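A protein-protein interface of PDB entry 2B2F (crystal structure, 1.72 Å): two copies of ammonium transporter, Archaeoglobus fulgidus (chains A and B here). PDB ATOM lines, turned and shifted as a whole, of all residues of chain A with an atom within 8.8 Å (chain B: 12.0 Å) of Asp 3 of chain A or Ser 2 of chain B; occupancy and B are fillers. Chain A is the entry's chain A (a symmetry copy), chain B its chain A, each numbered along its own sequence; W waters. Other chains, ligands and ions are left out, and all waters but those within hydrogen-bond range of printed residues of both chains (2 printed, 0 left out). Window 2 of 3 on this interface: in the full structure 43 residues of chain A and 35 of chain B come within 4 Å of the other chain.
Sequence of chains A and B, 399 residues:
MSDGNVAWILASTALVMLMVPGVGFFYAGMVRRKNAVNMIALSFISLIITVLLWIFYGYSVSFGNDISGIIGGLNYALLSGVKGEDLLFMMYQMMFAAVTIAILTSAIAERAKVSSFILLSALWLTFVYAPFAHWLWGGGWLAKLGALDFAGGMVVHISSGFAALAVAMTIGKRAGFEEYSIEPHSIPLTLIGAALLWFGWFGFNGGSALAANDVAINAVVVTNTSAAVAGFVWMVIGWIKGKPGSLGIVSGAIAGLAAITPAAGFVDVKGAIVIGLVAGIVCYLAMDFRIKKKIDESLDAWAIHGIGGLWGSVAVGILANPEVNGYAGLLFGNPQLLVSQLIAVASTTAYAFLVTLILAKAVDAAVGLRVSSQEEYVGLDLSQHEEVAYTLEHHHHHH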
ATOM      1  N   MET A   1      29.725 -28.373 -36.887  1.00  0.00           N
ATOM      2  CA  MET A   1      29.911 -26.900 -36.691  1.00  0.00           C
ATOM      3  C   MET A   1      30.740 -26.654 -35.450  1.00  0.00           C
ATOM      4  O   MET A   1      31.069 -25.514 -35.133  1.00  0.00           O
ATOM      5  CB  MET A   1      28.559 -26.207 -36.496  1.00  0.00           C
ATOM      6  CG  MET A   1      27.586 -26.320 -37.653  1.00  0.00           C
ATOM      7  SD  MET A   1      26.132 -25.290 -37.310  1.00  0.00           S
ATOM      8  CE  MET A   1      25.257 -26.354 -36.117  1.00  0.00           C
ATOM      9  N   SER A   2      31.105 -27.742 -34.783  1.00  0.00           N
ATOM     10  CA  SER A   2      31.831 -27.696 -33.527  1.00  0.00           C
ATOM     11  C   SER A   2      30.710 -27.376 -32.561  1.00  0.00           C
ATOM     12  O   SER A   2      30.282 -26.223 -32.428  1.00  0.00           O
ATOM     13  CB  SER A   2      32.875 -26.586 -33.477  1.00  0.00           C
ATOM     14  OG  SER A   2      33.358 -26.460 -32.152  1.00  0.00           O
ATOM     15  N   ASP A   3      30.206 -28.420 -31.924  1.00  0.00           N
ATOM     16  CA  ASP A   3      29.126 -28.278 -30.972  1.00  0.00           C
ATOM     17  C   ASP A   3      29.554 -27.327 -29.876  1.00  0.00           C
ATOM     18  O   ASP A   3      28.750 -26.551 -29.365  1.00  0.00           O
ATOM     19  CB  ASP A   3      28.787 -29.634 -30.371  1.00  0.00           C
ATOM     20  CG  ASP A   3      28.444 -30.665 -31.428  1.00  0.00           C
ATOM     21  OD1 ASP A   3      28.075 -30.262 -32.552  1.00  0.00           O
ATOM     22  OD2 ASP A   3      28.532 -31.879 -31.135  1.00  0.00           O
ATOM     23  N   GLY A   4      30.832 -27.401 -29.519  1.00  0.00           N
ATOM     24  CA  GLY A   4      31.350 -26.549 -28.474  1.00  0.00           C
ATOM     25  C   GLY A   4      31.197 -25.090 -28.826  1.00  0.00           C
ATOM     26  O   GLY A   4      30.768 -24.291 -27.996  1.00  0.00           O
ATOM     27  N   ASN A   5      31.540 -24.732 -30.059  1.00  0.00           N
ATOM     28  CA  ASN A   5      31.428 -23.346 -30.479  1.00  0.00           C
ATOM     29  C   ASN A   5      29.978 -22.907 -30.554  1.00  0.00           C
ATOM     30  O   ASN A   5      29.641 -21.794 -30.153  1.00  0.00           O
ATOM     31  CB  ASN A   5      32.097 -23.134 -31.830  1.00  0.00           C
ATOM     32  CG  ASN A   5      33.603 -23.230 -31.748  1.00  0.00           C
ATOM     33  OD1 ASN A   5      34.186 -23.116 -30.664  1.00  0.00           O
ATOM     34  ND2 ASN A   5      34.249 -23.421 -32.895  1.00  0.00           N
ATOM     35  N   VAL A   6      29.115 -23.769 -31.075  1.00  0.00           N
ATOM     36  CA  VAL A   6      27.701 -23.429 -31.156  1.00  0.00           C
ATOM     37  C   VAL A   6      27.171 -23.249 -29.732  1.00  0.00           C
ATOM     38  O   VAL A   6      26.429 -22.312 -29.444  1.00  0.00           O
ATOM     39  CB  VAL A   6      26.897 -24.544 -31.868  1.00  0.00           C
ATOM     40  CG1 VAL A   6      25.401 -24.266 -31.770  1.00  0.00           C
ATOM     41  CG2 VAL A   6      27.328 -24.636 -33.326  1.00  0.00           C
ATOM     42  N   ALA A   7      27.574 -24.146 -28.842  1.00  0.00           N
ATOM     43  CA  ALA A   7      27.139 -24.085 -27.456  1.00  0.00           C
ATOM     44  C   ALA A   7      27.467 -22.732 -26.851  1.00  0.00           C
ATOM     45  O   ALA A   7      26.599 -22.067 -26.282  1.00  0.00           O
ATOM     46  CB  ALA A   7      27.810 -25.181 -26.647  1.00  0.00           C
ATOM     47  N   TRP A   8      28.720 -22.323 -26.987  1.00  0.00           N
ATOM     48  CA  TRP A   8      29.149 -21.061 -26.422  1.00  0.00           C
ATOM     49  C   TRP A   8      28.411 -19.864 -27.005  1.00  0.00           C
ATOM     50  O   TRP A   8      28.044 -18.946 -26.276  1.00  0.00           O
ATOM     51  CB  TRP A   8      30.649 -20.885 -26.613  1.00  0.00           C
ATOM     52  CG  TRP A   8      31.157 -19.598 -26.066  1.00  0.00           C
ATOM     53  CD1 TRP A   8      31.989 -18.721 -26.692  1.00  0.00           C
ATOM     54  CD2 TRP A   8      30.842 -19.014 -24.790  1.00  0.00           C
ATOM     55  NE1 TRP A   8      32.212 -17.621 -25.891  1.00  0.00           N
ATOM     56  CE2 TRP A   8      31.518 -17.778 -24.720  1.00  0.00           C
ATOM     57  CE3 TRP A   8      30.051 -19.416 -23.704  1.00  0.00           C
ATOM     58  CZ2 TRP A   8      31.429 -16.935 -23.604  1.00  0.00           C
ATOM     59  CZ3 TRP A   8      29.961 -18.573 -22.592  1.00  0.00           C
ATOM     60  CH2 TRP A   8      30.646 -17.348 -22.555  1.00  0.00           C
ATOM     61  N   ILE A   9      28.173 -19.857 -28.308  1.00  0.00           N
ATOM     62  CA  ILE A   9      27.476 -18.716 -28.885  1.00  0.00           C
ATOM     63  C   ILE A   9      25.990 -18.729 -28.552  1.00  0.00           C
ATOM     64  O   ILE A   9      25.366 -17.673 -28.427  1.00  0.00           O
ATOM     65  CB  ILE A   9      27.684 -18.643 -30.399  1.00  0.00           C
ATOM     66  CG1 ILE A   9      29.187 -18.575 -30.689  1.00  0.00           C
ATOM     67  CG2 ILE A   9      27.017 -17.402 -30.972  1.00  0.00           C
ATOM     68  CD1 ILE A   9      29.917 -17.488 -29.905  1.00  0.00           C
ATOM     69  N   LEU A  10      25.418 -19.919 -28.407  1.00  0.00           N
ATOM     70  CA  LEU A  10      24.012 -20.014 -28.033  1.00  0.00           C
ATOM     71  C   LEU A  10      23.923 -19.352 -26.656  1.00  0.00           C
ATOM     72  O   LEU A  10      23.096 -18.468 -26.422  1.00  0.00           O
ATOM     73  CB  LEU A  10      23.581 -21.479 -27.954  1.00  0.00           C
ATOM     74  CG  LEU A  10      23.209 -22.119 -29.293  1.00  0.00           C
ATOM     75  CD1 LEU A  10      22.951 -23.606 -29.144  1.00  0.00           C
ATOM     76  CD2 LEU A  10      21.967 -21.428 -29.812  1.00  0.00           C
ATOM     77  N   ALA A  11      24.806 -19.770 -25.760  1.00  0.00           N
ATOM     78  CA  ALA A  11      24.845 -19.213 -24.420  1.00  0.00           C
ATOM     79  C   ALA A  11      25.104 -17.710 -24.456  1.00  0.00           C
ATOM     80  O   ALA A  11      24.405 -16.940 -23.794  1.00  0.00           O
ATOM     81  CB  ALA A  11      25.919 -19.903 -23.601  1.00  0.00           C
ATOM     82  N   GLU A  85      24.844 -21.874 -39.344  1.00  0.00           N
ATOM     83  CA  GLU A  85      25.587 -20.960 -38.488  1.00  0.00           C
ATOM     84  C   GLU A  85      25.281 -19.496 -38.754  1.00  0.00           C
ATOM     85  O   GLU A  85      25.444 -18.661 -37.867  1.00  0.00           O
ATOM     86  CB  GLU A  85      27.090 -21.212 -38.622  1.00  0.00           C
ATOM     87  CG  GLU A  85      27.510 -22.599 -38.138  1.00  0.00           C
ATOM     88  CD  GLU A  85      29.024 -22.811 -38.156  1.00  0.00           C
ATOM     89  OE1 GLU A  85      29.686 -22.219 -39.043  1.00  0.00           O
ATOM     90  OE2 GLU A  85      29.546 -23.575 -37.301  1.00  0.00           O
ATOM     91  N   LEU A  88      22.660 -18.412 -36.414  1.00  0.00           N
ATOM     92  CA  LEU A  88      23.138 -18.151 -35.064  1.00  0.00           C
ATOM     93  C   LEU A  88      23.777 -16.761 -34.990  1.00  0.00           C
ATOM     94  O   LEU A  88      23.552 -16.016 -34.032  1.00  0.00           O
ATOM     95  CB  LEU A  88      24.141 -19.235 -34.641  1.00  0.00           C
ATOM     96  CG  LEU A  88      24.688 -19.164 -33.204  1.00  0.00           C
ATOM     97  CD1 LEU A  88      23.557 -18.897 -32.238  1.00  0.00           C
ATOM     98  CD2 LEU A  88      25.398 -20.461 -32.843  1.00  0.00           C
ATOM     99  N   ALA A 212      34.580 -20.959 -28.920  1.00  0.00           N
ATOM    100  CA  ALA A 212      35.029 -21.184 -27.550  1.00  0.00           C
ATOM    101  C   ALA A 212      36.524 -21.478 -27.678  1.00  0.00           C
ATOM    102  O   ALA A 212      36.952 -22.621 -27.525  1.00  0.00           O
ATOM    103  CB  ALA A 212      34.293 -22.386 -26.941  1.00  0.00           C
ATOM    104  N   MET B   1      30.792 -37.845 -25.654  1.00  0.00           N
ATOM    105  CA  MET B   1      29.340 -37.481 -25.647  1.00  0.00           C
ATOM    106  C   MET B   1      29.135 -36.197 -26.420  1.00  0.00           C
ATOM    107  O   MET B   1      28.005 -35.747 -26.596  1.00  0.00           O
ATOM    108  CB  MET B   1      28.848 -37.250 -24.215  1.00  0.00           C
ATOM    109  CG  MET B   1      28.951 -38.441 -23.281  1.00  0.00           C
ATOM    110  SD  MET B   1      28.157 -38.027 -21.703  1.00  0.00           S
ATOM    111  CE  MET B   1      29.450 -36.985 -20.954  1.00  0.00           C
ATOM    112  N   SER B   2      30.237 -35.645 -26.911  1.00  0.00           N
ATOM    113  CA  SER B   2      30.243 -34.371 -27.607  1.00  0.00           C
ATOM    114  C   SER B   2      30.178 -33.408 -26.441  1.00  0.00           C
ATOM    115  O   SER B   2      29.111 -33.161 -25.867  1.00  0.00           O
ATOM    116  CB  SER B   2      29.024 -34.169 -28.500  1.00  0.00           C
ATOM    117  OG  SER B   2      28.989 -32.824 -28.944  1.00  0.00           O
ATOM    118  N   ASP B   3      31.343 -32.906 -26.065  1.00  0.00           N
ATOM    119  CA  ASP B   3      31.446 -31.976 -24.963  1.00  0.00           C
ATOM    120  C   ASP B   3      30.580 -30.769 -25.249  1.00  0.00           C
ATOM    121  O   ASP B   3      29.975 -30.198 -24.345  1.00  0.00           O
ATOM    122  CB  ASP B   3      32.894 -31.539 -24.790  1.00  0.00           C
ATOM    123  CG  ASP B   3      33.833 -32.714 -24.598  1.00  0.00           C
ATOM    124  OD1 ASP B   3      33.354 -33.795 -24.196  1.00  0.00           O
ATOM    125  OD2 ASP B   3      35.051 -32.554 -24.836  1.00  0.00           O
ATOM    126  N   GLY B   4      30.534 -30.386 -26.520  1.00  0.00           N
ATOM    127  CA  GLY B   4      29.747 -29.238 -26.911  1.00  0.00           C
ATOM    128  C   GLY B   4      28.289 -29.431 -26.577  1.00  0.00           C
ATOM    129  O   GLY B   4      27.649 -28.529 -26.038  1.00  0.00           O
ATOM    130  N   ASN B   5      27.753 -30.606 -26.890  1.00  0.00           N
ATOM    131  CA  ASN B   5      26.354 -30.872 -26.607  1.00  0.00           C
ATOM    132  C   ASN B   5      26.094 -30.940 -25.114  1.00  0.00           C
ATOM    133  O   ASN B   5      25.084 -30.428 -24.633  1.00  0.00           O
ATOM    134  CB  ASN B   5      25.907 -32.172 -27.263  1.00  0.00           C
ATOM    135  CG  ASN B   5      25.822 -32.057 -28.768  1.00  0.00           C
ATOM    136  OD1 ASN B   5      25.759 -30.951 -29.316  1.00  0.00           O
ATOM    137  ND2 ASN B   5      25.798 -33.200 -29.449  1.00  0.00           N
ATOM    138  N   VAL B   6      26.993 -31.577 -24.376  1.00  0.00           N
ATOM    139  CA  VAL B   6      26.825 -31.662 -22.932  1.00  0.00           C
ATOM    140  C   VAL B   6      26.876 -30.242 -22.362  1.00  0.00           C
ATOM    141  O   VAL B   6      26.079 -29.873 -21.503  1.00  0.00           O
ATOM    142  CB  VAL B   6      27.945 -32.515 -22.288  1.00  0.00           C
ATOM    143  CG1 VAL B   6      27.869 -32.431 -20.767  1.00  0.00           C
ATOM    144  CG2 VAL B   6      27.815 -33.963 -22.747  1.00  0.00           C
ATOM    145  N   ALA B   7      27.811 -29.446 -22.864  1.00  0.00           N
ATOM    146  CA  ALA B   7      27.962 -28.075 -22.405  1.00  0.00           C
ATOM    147  C   ALA B   7      26.657 -27.314 -22.548  1.00  0.00           C
ATOM    148  O   ALA B   7      26.175 -26.700 -21.595  1.00  0.00           O
ATOM    149  CB  ALA B   7      29.050 -27.374 -23.199  1.00  0.00           C
ATOM    150  N   TRP B   8      26.081 -27.368 -23.741  1.00  0.00           N
ATOM    151  CA  TRP B   8      24.848 -26.655 -23.996  1.00  0.00           C
ATOM    152  C   TRP B   8      23.695 -27.122 -23.120  1.00  0.00           C
ATOM    153  O   TRP B   8      22.919 -26.306 -22.629  1.00  0.00           O
ATOM    154  CB  TRP B   8      24.465 -26.781 -25.465  1.00  0.00           C
ATOM    155  CG  TRP B   8      23.194 -26.080 -25.796  1.00  0.00           C
ATOM    156  CD1 TRP B   8      22.155 -26.581 -26.518  1.00  0.00           C
ATOM    157  CD2 TRP B   8      22.804 -24.758 -25.390  1.00  0.00           C
ATOM    158  NE1 TRP B   8      21.134 -25.657 -26.587  1.00  0.00           N
ATOM    159  CE2 TRP B   8      21.509 -24.531 -25.902  1.00  0.00           C
ATOM    160  CE3 TRP B   8      23.423 -23.746 -24.641  1.00  0.00           C
ATOM    161  CZ2 TRP B   8      20.816 -23.332 -25.689  1.00  0.00           C
ATOM    162  CZ3 TRP B   8      22.730 -22.550 -24.428  1.00  0.00           C
ATOM    163  CH2 TRP B   8      21.441 -22.358 -24.951  1.00  0.00           C
ATOM    164  N   ILE B   9      23.569 -28.423 -22.902  1.00  0.00           N
ATOM    165  CA  ILE B   9      22.467 -28.890 -22.073  1.00  0.00           C
ATOM    166  C   ILE B   9      22.704 -28.603 -20.597  1.00  0.00           C
ATOM    167  O   ILE B   9      21.755 -28.379 -19.840  1.00  0.00           O
ATOM    168  CB  ILE B   9      22.197 -30.379 -22.292  1.00  0.00           C
ATOM    169  CG1 ILE B   9      21.907 -30.617 -23.778  1.00  0.00           C
ATOM    170  CG2 ILE B   9      20.992 -30.830 -21.480  1.00  0.00           C
ATOM    171  CD1 ILE B   9      20.834 -29.695 -24.352  1.00  0.00           C
ATOM    172  N   LEU B  10      23.965 -28.607 -20.179  1.00  0.00           N
ATOM    173  CA  LEU B  10      24.277 -28.287 -18.791  1.00  0.00           C
ATOM    174  C   LEU B  10      23.793 -26.848 -18.599  1.00  0.00           C
ATOM    175  O   LEU B  10      23.052 -26.541 -17.663  1.00  0.00           O
ATOM    176  CB  LEU B  10      25.784 -28.382 -18.550  1.00  0.00           C
ATOM    177  CG  LEU B  10      26.309 -29.795 -18.282  1.00  0.00           C
ATOM    178  CD1 LEU B  10      27.824 -29.819 -18.215  1.00  0.00           C
ATOM    179  CD2 LEU B  10      25.725 -30.269 -16.970  1.00  0.00           C
ATOM    180  N   ALA B  11      24.196 -25.978 -19.515  1.00  0.00           N
ATOM    181  CA  ALA B  11      23.794 -24.584 -19.463  1.00  0.00           C
ATOM    182  C   ALA B  11      22.277 -24.446 -19.528  1.00  0.00           C
ATOM    183  O   ALA B  11      21.680 -23.723 -18.727  1.00  0.00           O
ATOM    184  CB  ALA B  11      24.433 -23.817 -20.605  1.00  0.00           C
ATOM    185  N   SER B  12      21.644 -25.134 -20.471  1.00  0.00           N
ATOM    186  CA  SER B  12      20.204 -25.032 -20.605  1.00  0.00           C
ATOM    187  C   SER B  12      19.498 -25.455 -19.327  1.00  0.00           C
ATOM    188  O   SER B  12      18.458 -24.892 -18.971  1.00  0.00           O
ATOM    189  CB  SER B  12      19.723 -25.875 -21.782  1.00  0.00           C
ATOM    190  OG  SER B  12      20.201 -25.334 -22.999  1.00  0.00           O
ATOM    191  N   GLY B  84      25.373 -41.590 -17.067  1.00  0.00           N
ATOM    192  CA  GLY B  84      25.855 -40.822 -18.200  1.00  0.00           C
ATOM    193  C   GLY B  84      24.882 -39.775 -18.701  1.00  0.00           C
ATOM    194  O   GLY B  84      24.283 -39.045 -17.914  1.00  0.00           O
ATOM    195  N   GLU B  85      24.720 -39.705 -20.018  1.00  0.00           N
ATOM    196  CA  GLU B  85      23.824 -38.732 -20.626  1.00  0.00           C
ATOM    197  C   GLU B  85      22.389 -38.843 -20.140  1.00  0.00           C
ATOM    198  O   GLU B  85      21.646 -37.864 -20.180  1.00  0.00           O
ATOM    199  CB  GLU B  85      23.868 -38.850 -22.150  1.00  0.00           C
ATOM    200  CG  GLU B  85      25.238 -38.511 -22.737  1.00  0.00           C
ATOM    201  CD  GLU B  85      25.254 -38.509 -24.266  1.00  0.00           C
ATOM    202  OE1 GLU B  85      24.487 -39.305 -24.860  1.00  0.00           O
ATOM    203  OE2 GLU B  85      26.039 -37.729 -24.869  1.00  0.00           O
ATOM    204  N   ASP B  86      21.986 -40.027 -19.690  1.00  0.00           N
ATOM    205  CA  ASP B  86      20.627 -40.190 -19.191  1.00  0.00           C
ATOM    206  C   ASP B  86      20.457 -39.363 -17.933  1.00  0.00           C
ATOM    207  O   ASP B  86      19.365 -38.875 -17.648  1.00  0.00           O
ATOM    208  CB  ASP B  86      20.321 -41.654 -18.894  1.00  0.00           C
ATOM    209  CG  ASP B  86      19.998 -42.438 -20.142  1.00  0.00           C
ATOM    210  OD1 ASP B  86      19.490 -43.567 -20.005  1.00  0.00           O
ATOM    211  OD2 ASP B  86      20.249 -41.931 -21.255  1.00  0.00           O
ATOM    212  N   LEU B  88      21.915 -36.473 -17.367  1.00  0.00           N
ATOM    213  CA  LEU B  88      21.752 -35.090 -17.788  1.00  0.00           C
ATOM    214  C   LEU B  88      20.310 -34.843 -18.243  1.00  0.00           C
ATOM    215  O   LEU B  88      19.712 -33.815 -17.912  1.00  0.00           O
ATOM    216  CB  LEU B  88      22.742 -34.761 -18.915  1.00  0.00           C
ATOM    217  CG  LEU B  88      22.766 -33.310 -19.428  1.00  0.00           C
ATOM    218  CD1 LEU B  88      22.755 -32.353 -18.258  1.00  0.00           C
ATOM    219  CD2 LEU B  88      23.997 -33.075 -20.293  1.00  0.00           C
ATOM    220  N   PHE B  89      19.758 -35.790 -18.999  1.00  0.00           N
ATOM    221  CA  PHE B  89      18.393 -35.685 -19.495  1.00  0.00           C
ATOM    222  C   PHE B  89      17.429 -35.644 -18.318  1.00  0.00           C
ATOM    223  O   PHE B  89      16.490 -34.848 -18.285  1.00  0.00           O
ATOM    224  CB  PHE B  89      18.065 -36.886 -20.377  1.00  0.00           C
ATOM    225  CG  PHE B  89      16.655 -36.889 -20.893  1.00  0.00           C
ATOM    226  CD1 PHE B  89      16.264 -36.016 -21.905  1.00  0.00           C
ATOM    227  CD2 PHE B  89      15.709 -37.756 -20.357  1.00  0.00           C
ATOM    228  CE1 PHE B  89      14.948 -36.009 -22.377  1.00  0.00           C
ATOM    229  CE2 PHE B  89      14.391 -37.756 -20.820  1.00  0.00           C
ATOM    230  CZ  PHE B  89      14.010 -36.882 -21.832  1.00  0.00           C
ATOM    231  N   GLY B 206      15.636 -23.818 -26.647  1.00  0.00           N
ATOM    232  CA  GLY B 206      16.909 -24.115 -27.280  1.00  0.00           C
ATOM    233  C   GLY B 206      17.582 -25.397 -26.823  1.00  0.00           C
ATOM    234  O   GLY B 206      18.294 -26.042 -27.596  1.00  0.00           O
ATOM    235  N   GLY B 207      17.368 -25.773 -25.569  1.00  0.00           N
ATOM    236  CA  GLY B 207      17.988 -26.983 -25.065  1.00  0.00           C
ATOM    237  C   GLY B 207      17.197 -28.227 -25.413  1.00  0.00           C
ATOM    238  O   GLY B 207      17.707 -29.337 -25.292  1.00  0.00           O
ATOM    239  N   ALA B 209      16.562 -29.502 -28.140  1.00  0.00           N
ATOM    240  CA  ALA B 209      17.083 -30.230 -29.297  1.00  0.00           C
ATOM    241  C   ALA B 209      18.067 -31.261 -28.749  1.00  0.00           C
ATOM    242  O   ALA B 209      18.510 -32.170 -29.457  1.00  0.00           O
ATOM    243  CB  ALA B 209      17.801 -29.277 -30.249  1.00  0.00           C
ATOM    244  N   LEU B 210      18.397 -31.090 -27.472  1.00  0.00           N
ATOM    245  CA  LEU B 210      19.319 -31.949 -26.744  1.00  0.00           C
ATOM    246  C   LEU B 210      20.700 -32.000 -27.375  1.00  0.00           C
ATOM    247  O   LEU B 210      21.440 -32.969 -27.201  1.00  0.00           O
ATOM    248  CB  LEU B 210      18.731 -33.353 -26.603  1.00  0.00           C
ATOM    249  CG  LEU B 210      17.418 -33.364 -25.809  1.00  0.00           C
ATOM    250  CD1 LEU B 210      16.886 -34.782 -25.696  1.00  0.00           C
ATOM    251  CD2 LEU B 210      17.650 -32.793 -24.417  1.00  0.00           C
ATOM    252  N   ALA B 211      21.044 -30.928 -28.083  1.00  0.00           N
ATOM    253  CA  ALA B 211      22.334 -30.799 -28.746  1.00  0.00           C
ATOM    254  C   ALA B 211      22.524 -29.358 -29.198  1.00  0.00           C
ATOM    255  O   ALA B 211      21.545 -28.615 -29.356  1.00  0.00           O
ATOM    256  CB  ALA B 211      22.403 -31.719 -29.950  1.00  0.00           C
ATOM    257  N   ALA B 212      23.782 -28.968 -29.406  1.00  0.00           N
ATOM    258  CA  ALA B 212      24.104 -27.619 -29.860  1.00  0.00           C
ATOM    259  C   ALA B 212      24.191 -27.736 -31.381  1.00  0.00           C
ATOM    260  O   ALA B 212      25.282 -27.698 -31.950  1.00  0.00           O
ATOM    261  CB  ALA B 212      25.449 -27.169 -29.275  1.00  0.00           C
ATOM    262  N   ASN B 213      23.033 -27.879 -32.029  1.00  0.00           N
ATOM    263  CA  ASN B 213      22.950 -28.046 -33.482  1.00  0.00           C
ATOM    264  C   ASN B 213      22.043 -27.047 -34.194  1.00  0.00           C
ATOM    265  O   ASN B 213      21.583 -26.069 -33.600  1.00  0.00           O
ATOM    266  CB  ASN B 213      22.477 -29.466 -33.806  1.00  0.00           C
ATOM    267  CG  ASN B 213      21.085 -29.767 -33.258  1.00  0.00           C
ATOM    268  OD1 ASN B 213      20.649 -30.920 -33.242  1.00  0.00           O
ATOM    269  ND2 ASN B 213      20.381 -28.734 -32.819  1.00  0.00           N
ATOM    270  N   ASP B 214      21.779 -27.302 -35.474  1.00  0.00           N
ATOM    271  CA  ASP B 214      20.925 -26.417 -36.267  1.00  0.00           C
ATOM    272  C   ASP B 214      19.488 -26.327 -35.740  1.00  0.00           C
ATOM    273  O   ASP B 214      18.822 -25.298 -35.898  1.00  0.00           O
ATOM    274  CB  ASP B 214      20.908 -26.866 -37.739  1.00  0.00           C
ATOM    275  CG  ASP B 214      22.163 -26.447 -38.504  1.00  0.00           C
ATOM    276  OD1 ASP B 214      22.332 -26.901 -39.660  1.00  0.00           O
ATOM    277  OD2 ASP B 214      22.970 -25.662 -37.958  1.00  0.00           O
ATOM    278  N   VAL B 215      19.000 -27.396 -35.118  1.00  0.00           N
ATOM    279  CA  VAL B 215      17.640 -27.374 -34.590  1.00  0.00           C
ATOM    280  C   VAL B 215      17.559 -26.460 -33.367  1.00  0.00           C
ATOM    281  O   VAL B 215      16.580 -25.733 -33.189  1.00  0.00           O
ATOM    282  CB  VAL B 215      17.147 -28.791 -34.218  1.00  0.00           C
ATOM    283  CG1 VAL B 215      15.803 -28.704 -33.504  1.00  0.00           C
ATOM    284  CG2 VAL B 215      16.992 -29.629 -35.484  1.00  0.00           C
ATOM    285  N   ALA B 216      18.588 -26.494 -32.525  1.00  0.00           N
ATOM    286  CA  ALA B 216      18.615 -25.638 -31.335  1.00  0.00           C
ATOM    287  C   ALA B 216      18.657 -24.176 -31.803  1.00  0.00           C
ATOM    288  O   ALA B 216      17.951 -23.311 -31.274  1.00  0.00           O
ATOM    289  CB  ALA B 216      19.853 -25.953 -30.480  1.00  0.00           C
ATOM    290  N   ILE B 217      19.496 -23.909 -32.800  1.00  0.00           N
ATOM    291  CA  ILE B 217      19.631 -22.567 -33.345  1.00  0.00           C
ATOM    292  C   ILE B 217      18.283 -22.083 -33.877  1.00  0.00           C
ATOM    293  O   ILE B 217      17.873 -20.947 -33.635  1.00  0.00           O
ATOM    294  CB  ILE B 217      20.678 -22.550 -34.475  1.00  0.00           C
ATOM    295  CG1 ILE B 217      22.064 -22.845 -33.896  1.00  0.00           C
ATOM    296  CG2 ILE B 217      20.662 -21.213 -35.185  1.00  0.00           C
ATOM    297  CD1 ILE B 217      23.174 -22.924 -34.939  1.00  0.00           C
HETATM  298  O   HOH W   1      25.166 -31.300 -32.060  1.00  0.00           O
HETATM  299  O   HOH W   2      27.020 -28.517 -34.175  1.00  0.00           O
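OD2 of Asp 3 of chain A sits close to OD1 of Asn 5 of chain B, 3.4 Å away. The side-chain sulfur (SD) of Met 1 of chain A sits close to the side-chain carboxylate (OD2) of Asp 214 of chain B, at 3.2 Å. The side-chain hydroxyl (OG) of Ser 2 of chain B is in hydrogen-bond range of the side-chain carboxylate (OD2) of Asp 3 of chain A (2.4 Å).
The indole nitrogen of Trp 8 of chain B is in hydrogen-bond range of the backbone carbonyl oxygen of Gly 206 of chain B, at 3.0 Å. OD1 of Asn 5 of chain B sits at hydrogen-bond distance from N of Ala 212 of chain B (2.8 Å).
Among the printed residues, pairs that only touch across the chains: Met 1 of chain A with Asn 213 of chain B (3.8 Å), Asp 3 of chain A with Gly 4 of chain B (3.5 Å), Asp 3 of chain A with Ala 212 of chain B (3.4 Å), Gly 4 of chain A with Gly 4 of chain B (3.4 Å), Val 6 of chain A with Ala 212 of chain B (3.4 Å), Ala 7 of chain A with Gly 4 of chain B (3.4 Å), Ala 7 of chain A with Trp 8 of chain B (3.9 Å), Ala 7 of chain A with Ala 212 of chain B (3.7 Å), Leu 10 of chain A with Trp 8 of chain B (3.7 Å), Ala 11 of chain A with Trp 8 of chain B (3.7 Å) and Leu 88 of chain A with Ile 217 of chain B (3.7 Å).
Of the printed residues of chain B, Met 1 of chain A touches Asn 213 and Asp 214. Of chain B, only Gly 4 (3.4 Å) comes within 4 Å of Gly 4 of chain A. No residue of chain B comes within 4 Å of Asn 5 of chain A. Of chain B, only Ala 212 comes within 4 Å of Val 6 of chain A. Ala 7 of chain A touches just these residues of chain B: Gly 4, Trp 8 and Ala 212. Printed residues of chain B within 4 Å of Leu 10 of chain A: Trp 8 (3.7 Å). Printed residues of chain B within 4 Å of Leu 88 of chain A: Ile 217. Gly 206 of chain B touches none of the printed residues of chain A. The nearest residue of chain B that does not touch Asp 3 of chain A is Asp 3 of chain B (5.5 Å). The nearest residue of chain A that does not touch Ser 2 of chain B is Gly 4 of chain A (5.8 Å). The nearest printed residue of chain A that does not touch Trp 8 of chain B is Asp 3 of chain A (5.8 Å).
Printed residues of chain B that touch a printed residue of chain A: Ser 2, Gly 4, Asn 5, Trp 8, Ala 212, Asn 213, Asp 214 and Ile 217. Hydrophobic or aromatic side chains of chain B that line the printed part of chain A: Trp 8, Ala 212 and Ile 217. Along chain B the printed residues that touch a printed residue of chain A span positions 2 to 217. Among the printed residues, no Asp or Glu carboxylate lies within 4 Å of a Lys or Arg side-chain nitrogen of the other chain.
Leu 10 of chain A touches Trp 8 of chain B, but with the chains exchanged Trp 8 of chain A does not touch Leu 10 of chain B (10.4 Å). Of the 14 pairs that touch across the chains among the printed residues, 1 has its exchanged pair printed and touching as well.
Water W2 bridges OD1 of Asp 3 of chain A (2.6 Å) and O of Ala 212 of chain B (2.9 Å). Water W1 bridges OD1 of Asn 5 of chain B (2.8 Å) and OD1 of Asp 3 of chain A (3.1 Å).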
